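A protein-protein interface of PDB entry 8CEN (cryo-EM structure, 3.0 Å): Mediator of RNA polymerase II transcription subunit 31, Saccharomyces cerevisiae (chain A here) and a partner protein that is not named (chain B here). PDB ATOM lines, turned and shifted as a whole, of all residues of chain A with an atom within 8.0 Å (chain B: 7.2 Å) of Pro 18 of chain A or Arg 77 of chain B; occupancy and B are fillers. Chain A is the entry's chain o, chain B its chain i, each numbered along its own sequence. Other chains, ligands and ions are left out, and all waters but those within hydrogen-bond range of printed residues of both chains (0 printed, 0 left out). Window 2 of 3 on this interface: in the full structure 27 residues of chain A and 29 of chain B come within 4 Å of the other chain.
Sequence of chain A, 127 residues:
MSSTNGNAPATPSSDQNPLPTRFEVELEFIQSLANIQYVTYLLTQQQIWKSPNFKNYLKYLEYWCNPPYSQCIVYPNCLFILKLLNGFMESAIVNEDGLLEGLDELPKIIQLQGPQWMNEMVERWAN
The side-chain carboxylate (OE1) of Glu 24 of chain A is in salt-bridge range of the guanidinium group (NH2) of Arg 77 of chain B, at 3.8 Å.
The backbone NH of Phe 79 of chain B sits at hydrogen-bond distance from the side-chain carboxylate of Glu 28 of chain A.
O of Ala 78 of chain B lies within hydrogen-bond range of NE1 of Trp 83 of chain B (2.8 Å).
The backbone carbonyl oxygen of Tyr 76 of chain B sits at hydrogen-bond distance from the backbone NH of Trp 83 of chain B (2.9 Å).
The side-chain hydroxyl (OG) of Ser 81 of chain B lies within hydrogen-bond range of the backbone carbonyl oxygen (O) of Ala 78 of chain B, 2.7 Å away.
OG1 of Thr 21 of chain A is in hydrogen-bond range of N of Glu 24 of chain A (3.2 Å).
Arg 77 of chain B touches Pro 18 of chain A (NH1 to CG, 3.8 Å).
NH2 of Arg 77 of chain B touches O of Leu 19 of chain A, 3.9 Å away.
Pro 71 of chain B touches Phe 23 of chain A (CG to CE2, 3.7 Å).
CG of Tyr 76 of chain B touches CE2 of Phe 23 of chain A, 3.98 Å away.
Tyr 76 of chain B touches Glu 24 of chain A (CA to OE2, 3.4 Å).
Leu 27 of chain A touches Tyr 76 of chain B (CD1 to CE2, 3.6 Å).
Ala 78 of chain B touches Leu 27 of chain A.
Ala 78 of chain B touches Glu 28 of chain A (C to OE2, 3.3 Å).
Pro 18 of chain A touches just one residue of chain B: Arg 77 (3.8 Å).
Of chain A, only Pro 18 (3.8 Å), Leu 19 (3.9 Å) and Glu 24 (3.3 Å) come within 4 Å of Arg 77 of chain B.
Of the printed residues of chain A, Tyr 76 of chain B touches Phe 23 (3.98 Å), Glu 24 (3.4 Å) and Leu 27 (3.6 Å).
Printed residues of chain A within 4 Å of Phe 79 of chain B: Glu 28 (2.4 Å).
Gln 75 of chain B touches none of the printed residues of chain A.
The nearest printed residue of chain B that does not touch Pro 18 of chain A is Ile 82 of chain B (9.1 Å).
Printed residues of chain A that touch a printed residue of chain B: Pro 18, Leu 19, Phe 23, Glu 24, Leu 27 and Glu 28.
Hydrophobic or aromatic side chains of chain A that line the printed part of chain B: Pro 18, Phe 23 and Leu 27.
Of the 10 printed residues of chain B, 5 touch a printed residue of chain A.
Among the printed residues, Asp or Glu carboxylates within 4 Å of a Lys or Arg side-chain nitrogen of the other chain: Glu 24 of chain A with Arg 77 of chain B (3.8 Å).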
ATOM      1  N   ASN A  17       1.475 -24.061 -20.577  1.00  0.00           N
ATOM      2  CA  ASN A  17       0.288 -24.326 -19.774  1.00  0.00           C
ATOM      3  C   ASN A  17       0.046 -25.831 -19.671  1.00  0.00           C
ATOM      4  O   ASN A  17      -0.536 -26.430 -20.576  1.00  0.00           O
ATOM      5  CB  ASN A  17      -0.932 -23.625 -20.372  1.00  0.00           C
ATOM      6  CG  ASN A  17      -2.181 -23.825 -19.543  1.00  0.00           C
ATOM      7  OD1 ASN A  17      -2.108 -24.016 -18.330  1.00  0.00           O
ATOM      8  ND2 ASN A  17      -3.338 -23.778 -20.192  1.00  0.00           N
ATOM      9  N   PRO A  18       0.503 -26.435 -18.576  1.00  0.00           N
ATOM     10  CA  PRO A  18       0.448 -27.895 -18.455  1.00  0.00           C
ATOM     11  C   PRO A  18      -0.972 -28.424 -18.313  1.00  0.00           C
ATOM     12  O   PRO A  18      -1.893 -27.733 -17.872  1.00  0.00           O
ATOM     13  CB  PRO A  18       1.263 -28.177 -17.186  1.00  0.00           C
ATOM     14  CG  PRO A  18       2.133 -26.976 -17.020  1.00  0.00           C
ATOM     15  CD  PRO A  18       1.303 -25.828 -17.499  1.00  0.00           C
ATOM     16  N   LEU A  19      -1.126 -29.686 -18.704  1.00  0.00           N
ATOM     17  CA  LEU A  19      -2.383 -30.392 -18.529  1.00  0.00           C
ATOM     18  C   LEU A  19      -2.588 -30.715 -17.048  1.00  0.00           C
ATOM     19  O   LEU A  19      -1.619 -30.810 -16.290  1.00  0.00           O
ATOM     20  CB  LEU A  19      -2.375 -31.674 -19.363  1.00  0.00           C
ATOM     21  CG  LEU A  19      -3.672 -32.384 -19.761  1.00  0.00           C
ATOM     22  CD1 LEU A  19      -4.486 -31.523 -20.714  1.00  0.00           C
ATOM     23  CD2 LEU A  19      -3.377 -33.740 -20.380  1.00  0.00           C
ATOM     24  N   PRO A  20      -3.842 -30.841 -16.603  1.00  0.00           N
ATOM     25  CA  PRO A  20      -4.099 -31.236 -15.212  1.00  0.00           C
ATOM     26  C   PRO A  20      -3.518 -32.593 -14.846  1.00  0.00           C
ATOM     27  O   PRO A  20      -3.382 -33.488 -15.681  1.00  0.00           O
ATOM     28  CB  PRO A  20      -5.628 -31.250 -15.131  1.00  0.00           C
ATOM     29  CG  PRO A  20      -6.047 -30.224 -16.106  1.00  0.00           C
ATOM     30  CD  PRO A  20      -5.039 -30.243 -17.223  1.00  0.00           C
ATOM     31  N   THR A  21      -3.143 -32.723 -13.577  1.00  0.00           N
ATOM     32  CA  THR A  21      -2.628 -33.970 -13.036  1.00  0.00           C
ATOM     33  C   THR A  21      -3.682 -34.644 -12.167  1.00  0.00           C
ATOM     34  O   THR A  21      -4.582 -33.996 -11.623  1.00  0.00           O
ATOM     35  CB  THR A  21      -1.354 -33.735 -12.219  1.00  0.00           C
ATOM     36  OG1 THR A  21      -1.702 -33.227 -10.926  1.00  0.00           O
ATOM     37  CG2 THR A  21      -0.450 -32.733 -12.917  1.00  0.00           C
ATOM     38  N   PHE A  23      -3.332 -36.077  -9.265  1.00  0.00           N
ATOM     39  CA  PHE A  23      -3.221 -35.627  -7.878  1.00  0.00           C
ATOM     40  C   PHE A  23      -3.993 -34.332  -7.655  1.00  0.00           C
ATOM     41  O   PHE A  23      -4.769 -34.219  -6.703  1.00  0.00           O
ATOM     42  CB  PHE A  23      -1.744 -35.448  -7.513  1.00  0.00           C
ATOM     43  CG  PHE A  23      -1.509 -34.921  -6.118  1.00  0.00           C
ATOM     44  CD1 PHE A  23      -1.452 -35.789  -5.040  1.00  0.00           C
ATOM     45  CD2 PHE A  23      -1.314 -33.564  -5.889  1.00  0.00           C
ATOM     46  CE1 PHE A  23      -1.229 -35.314  -3.762  1.00  0.00           C
ATOM     47  CE2 PHE A  23      -1.097 -33.086  -4.613  1.00  0.00           C
ATOM     48  CZ  PHE A  23      -1.051 -33.962  -3.549  1.00  0.00           C
ATOM     49  N   GLU A  24      -3.807 -33.352  -8.542  1.00  0.00           N
ATOM     50  CA  GLU A  24      -4.426 -32.045  -8.346  1.00  0.00           C
ATOM     51  C   GLU A  24      -5.934 -32.099  -8.564  1.00  0.00           C
ATOM     52  O   GLU A  24      -6.697 -31.488  -7.804  1.00  0.00           O
ATOM     53  CB  GLU A  24      -3.769 -31.024  -9.274  1.00  0.00           C
ATOM     54  CG  GLU A  24      -2.326 -30.735  -8.894  1.00  0.00           C
ATOM     55  CD  GLU A  24      -1.597 -29.875  -9.905  1.00  0.00           C
ATOM     56  OE1 GLU A  24      -2.264 -29.195 -10.704  1.00  0.00           O
ATOM     57  OE2 GLU A  24      -0.349 -29.884  -9.904  1.00  0.00           O
ATOM     58  N   VAL A  25      -6.382 -32.839  -9.585  1.00  0.00           N
ATOM     59  CA  VAL A  25      -7.817 -32.978  -9.831  1.00  0.00           C
ATOM     60  C   VAL A  25      -8.495 -33.711  -8.680  1.00  0.00           C
ATOM     61  O   VAL A  25      -9.560 -33.295  -8.203  1.00  0.00           O
ATOM     62  CB  VAL A  25      -8.063 -33.678 -11.180  1.00  0.00           C
ATOM     63  CG1 VAL A  25      -9.546 -33.912 -11.399  1.00  0.00           C
ATOM     64  CG2 VAL A  25      -7.511 -32.837 -12.309  1.00  0.00           C
ATOM     65  N   LEU A  27      -7.400 -33.910  -5.612  1.00  0.00           N
ATOM     66  CA  LEU A  27      -7.339 -33.026  -4.452  1.00  0.00           C
ATOM     67  C   LEU A  27      -8.463 -32.004  -4.478  1.00  0.00           C
ATOM     68  O   LEU A  27      -9.132 -31.777  -3.463  1.00  0.00           O
ATOM     69  CB  LEU A  27      -5.976 -32.332  -4.406  1.00  0.00           C
ATOM     70  CG  LEU A  27      -5.596 -31.482  -3.192  1.00  0.00           C
ATOM     71  CD1 LEU A  27      -4.154 -31.736  -2.811  1.00  0.00           C
ATOM     72  CD2 LEU A  27      -5.788 -30.009  -3.501  1.00  0.00           C
ATOM     73  N   GLU A  28      -8.692 -31.380  -5.634  1.00  0.00           N
ATOM     74  CA  GLU A  28      -9.768 -30.400  -5.728  1.00  0.00           C
ATOM     75  C   GLU A  28     -11.132 -31.052  -5.540  1.00  0.00           C
ATOM     76  O   GLU A  28     -11.999 -30.491  -4.857  1.00  0.00           O
ATOM     77  CB  GLU A  28      -9.698 -29.668  -7.062  1.00  0.00           C
ATOM     78  CG  GLU A  28      -8.658 -28.574  -7.092  1.00  0.00           C
ATOM     79  CD  GLU A  28      -8.871 -27.634  -8.248  1.00  0.00           C
ATOM     80  OE1 GLU A  28      -9.276 -28.118  -9.321  1.00  0.00           O
ATOM     81  OE2 GLU A  28      -8.639 -26.421  -8.086  1.00  0.00           O
ATOM     82  N   PRO B  71       3.455 -34.622  -5.792  1.00  0.00           N
ATOM     83  CA  PRO B  71       4.057 -33.894  -6.919  1.00  0.00           C
ATOM     84  C   PRO B  71       5.579 -33.929  -6.888  1.00  0.00           C
ATOM     85  O   PRO B  71       6.205 -33.781  -5.837  1.00  0.00           O
ATOM     86  CB  PRO B  71       3.528 -32.467  -6.739  1.00  0.00           C
ATOM     87  CG  PRO B  71       2.266 -32.629  -5.980  1.00  0.00           C
ATOM     88  CD  PRO B  71       2.480 -33.790  -5.064  1.00  0.00           C
ATOM     89  N   GLN B  75       5.154 -28.557  -6.012  1.00  0.00           N
ATOM     90  CA  GLN B  75       4.143 -27.518  -6.132  1.00  0.00           C
ATOM     91  C   GLN B  75       2.951 -28.086  -6.884  1.00  0.00           C
ATOM     92  O   GLN B  75       3.113 -28.773  -7.897  1.00  0.00           O
ATOM     93  CB  GLN B  75       4.674 -26.286  -6.869  1.00  0.00           C
ATOM     94  CG  GLN B  75       5.983 -25.744  -6.337  1.00  0.00           C
ATOM     95  CD  GLN B  75       6.538 -24.636  -7.206  1.00  0.00           C
ATOM     96  OE1 GLN B  75       7.476 -24.844  -7.975  1.00  0.00           O
ATOM     97  NE2 GLN B  75       5.957 -23.448  -7.091  1.00  0.00           N
ATOM     98  N   TYR B  76       1.756 -27.802  -6.384  1.00  0.00           N
ATOM     99  CA  TYR B  76       0.530 -28.242  -7.028  1.00  0.00           C
ATOM    100  C   TYR B  76      -0.449 -27.081  -7.127  1.00  0.00           C
ATOM    101  O   TYR B  76      -0.438 -26.163  -6.306  1.00  0.00           O
ATOM    102  CB  TYR B  76      -0.111 -29.431  -6.286  1.00  0.00           C
ATOM    103  CG  TYR B  76      -0.570 -29.150  -4.872  1.00  0.00           C
ATOM    104  CD1 TYR B  76       0.329 -29.160  -3.812  1.00  0.00           C
ATOM    105  CD2 TYR B  76      -1.905 -28.890  -4.595  1.00  0.00           C
ATOM    106  CE1 TYR B  76      -0.089 -28.911  -2.520  1.00  0.00           C
ATOM    107  CE2 TYR B  76      -2.331 -28.639  -3.305  1.00  0.00           C
ATOM    108  CZ  TYR B  76      -1.419 -28.654  -2.272  1.00  0.00           C
ATOM    109  OH  TYR B  76      -1.840 -28.403  -0.987  1.00  0.00           O
ATOM    110  N   ARG B  77      -1.296 -27.130  -8.144  1.00  0.00           N
ATOM    111  CA  ARG B  77      -2.263 -26.076  -8.397  1.00  0.00           C
ATOM    112  C   ARG B  77      -3.641 -26.516  -7.925  1.00  0.00           C
ATOM    113  O   ARG B  77      -4.074 -27.639  -8.199  1.00  0.00           O
ATOM    114  CB  ARG B  77      -2.307 -25.726  -9.883  1.00  0.00           C
ATOM    115  CG  ARG B  77      -1.129 -24.921 -10.381  1.00  0.00           C
ATOM    116  CD  ARG B  77      -1.235 -24.697 -11.876  1.00  0.00           C
ATOM    117  NE  ARG B  77      -1.654 -25.910 -12.568  1.00  0.00           N
ATOM    118  CZ  ARG B  77      -0.937 -26.532 -13.494  1.00  0.00           C
ATOM    119  NH1 ARG B  77       0.250 -26.084 -13.866  1.00  0.00           N
ATOM    120  NH2 ARG B  77      -1.424 -27.632 -14.060  1.00  0.00           N
ATOM    121  N   ALA B  78      -4.326 -25.626  -7.208  1.00  0.00           N
ATOM    122  CA  ALA B  78      -5.669 -25.906  -6.719  1.00  0.00           C
ATOM    123  C   ALA B  78      -6.396 -24.590  -6.497  1.00  0.00           C
ATOM    124  O   ALA B  78      -5.833 -23.669  -5.897  1.00  0.00           O
ATOM    125  CB  ALA B  78      -5.631 -26.720  -5.422  1.00  0.00           C
ATOM    126  N   PHE B  79      -7.639 -24.516  -6.986  1.00  0.00           N
ATOM    127  CA  PHE B  79      -8.535 -23.368  -6.805  1.00  0.00           C
ATOM    128  C   PHE B  79      -7.925 -22.075  -7.343  1.00  0.00           C
ATOM    129  O   PHE B  79      -8.097 -20.999  -6.767  1.00  0.00           O
ATOM    130  CB  PHE B  79      -8.943 -23.214  -5.339  1.00  0.00           C
ATOM    131  CG  PHE B  79      -9.329 -24.508  -4.686  1.00  0.00           C
ATOM    132  CD1 PHE B  79     -10.455 -25.200  -5.098  1.00  0.00           C
ATOM    133  CD2 PHE B  79      -8.555 -25.041  -3.668  1.00  0.00           C
ATOM    134  CE1 PHE B  79     -10.806 -26.398  -4.502  1.00  0.00           C
ATOM    135  CE2 PHE B  79      -8.902 -26.235  -3.067  1.00  0.00           C
ATOM    136  CZ  PHE B  79     -10.029 -26.914  -3.485  1.00  0.00           C
ATOM    137  N   GLY B  80      -7.224 -22.181  -8.467  1.00  0.00           N
ATOM    138  CA  GLY B  80      -6.595 -21.024  -9.082  1.00  0.00           C
ATOM    139  C   GLY B  80      -5.464 -20.421  -8.279  1.00  0.00           C
ATOM    140  O   GLY B  80      -5.339 -19.191  -8.218  1.00  0.00           O
ATOM    141  N   SER B  81      -4.635 -21.257  -7.660  1.00  0.00           N
ATOM    142  CA  SER B  81      -3.526 -20.776  -6.851  1.00  0.00           C
ATOM    143  C   SER B  81      -2.431 -21.831  -6.833  1.00  0.00           C
ATOM    144  O   SER B  81      -2.656 -22.994  -7.176  1.00  0.00           O
ATOM    145  CB  SER B  81      -3.975 -20.441  -5.425  1.00  0.00           C
ATOM    146  OG  SER B  81      -4.447 -21.597  -4.758  1.00  0.00           O
ATOM    147  N   ILE B  82      -1.238 -21.407  -6.429  1.00  0.00           N
ATOM    148  CA  ILE B  82      -0.074 -22.282  -6.337  1.00  0.00           C
ATOM    149  C   ILE B  82       0.120 -22.664  -4.879  1.00  0.00           C
ATOM    150  O   ILE B  82       0.085 -21.800  -3.996  1.00  0.00           O
ATOM    151  CB  ILE B  82       1.186 -21.596  -6.891  1.00  0.00           C
ATOM    152  CG1 ILE B  82       0.884 -20.887  -8.213  1.00  0.00           C
ATOM    153  CG2 ILE B  82       2.303 -22.611  -7.076  1.00  0.00           C
ATOM    154  CD1 ILE B  82       0.536 -21.815  -9.344  1.00  0.00           C
ATOM    155  N   TRP B  83       0.331 -23.951  -4.621  1.00  0.00           N
ATOM    156  CA  TRP B  83       0.576 -24.451  -3.281  1.00  0.00           C
ATOM    157  C   TRP B  83       1.849 -25.278  -3.302  1.00  0.00           C
ATOM    158  O   TRP B  83       2.252 -25.803  -4.343  1.00  0.00           O
ATOM    159  CB  TRP B  83      -0.575 -25.325  -2.764  1.00  0.00           C
ATOM    160  CG  TRP B  83      -1.959 -24.782  -2.954  1.00  0.00           C
ATOM    161  CD1 TRP B  83      -2.666 -24.725  -4.120  1.00  0.00           C
ATOM    162  CD2 TRP B  83      -2.823 -24.262  -1.938  1.00  0.00           C
ATOM    163  NE1 TRP B  83      -3.906 -24.182  -3.897  1.00  0.00           N
ATOM    164  CE2 TRP B  83      -4.028 -23.890  -2.564  1.00  0.00           C
ATOM    165  CE3 TRP B  83      -2.689 -24.064  -0.561  1.00  0.00           C
ATOM    166  CZ2 TRP B  83      -5.094 -23.336  -1.861  1.00  0.00           C
ATOM    167  CZ3 TRP B  83      -3.743 -23.508   0.133  1.00  0.00           C
ATOM    168  CH2 TRP B  83      -4.933 -23.156  -0.515  1.00  0.00           C
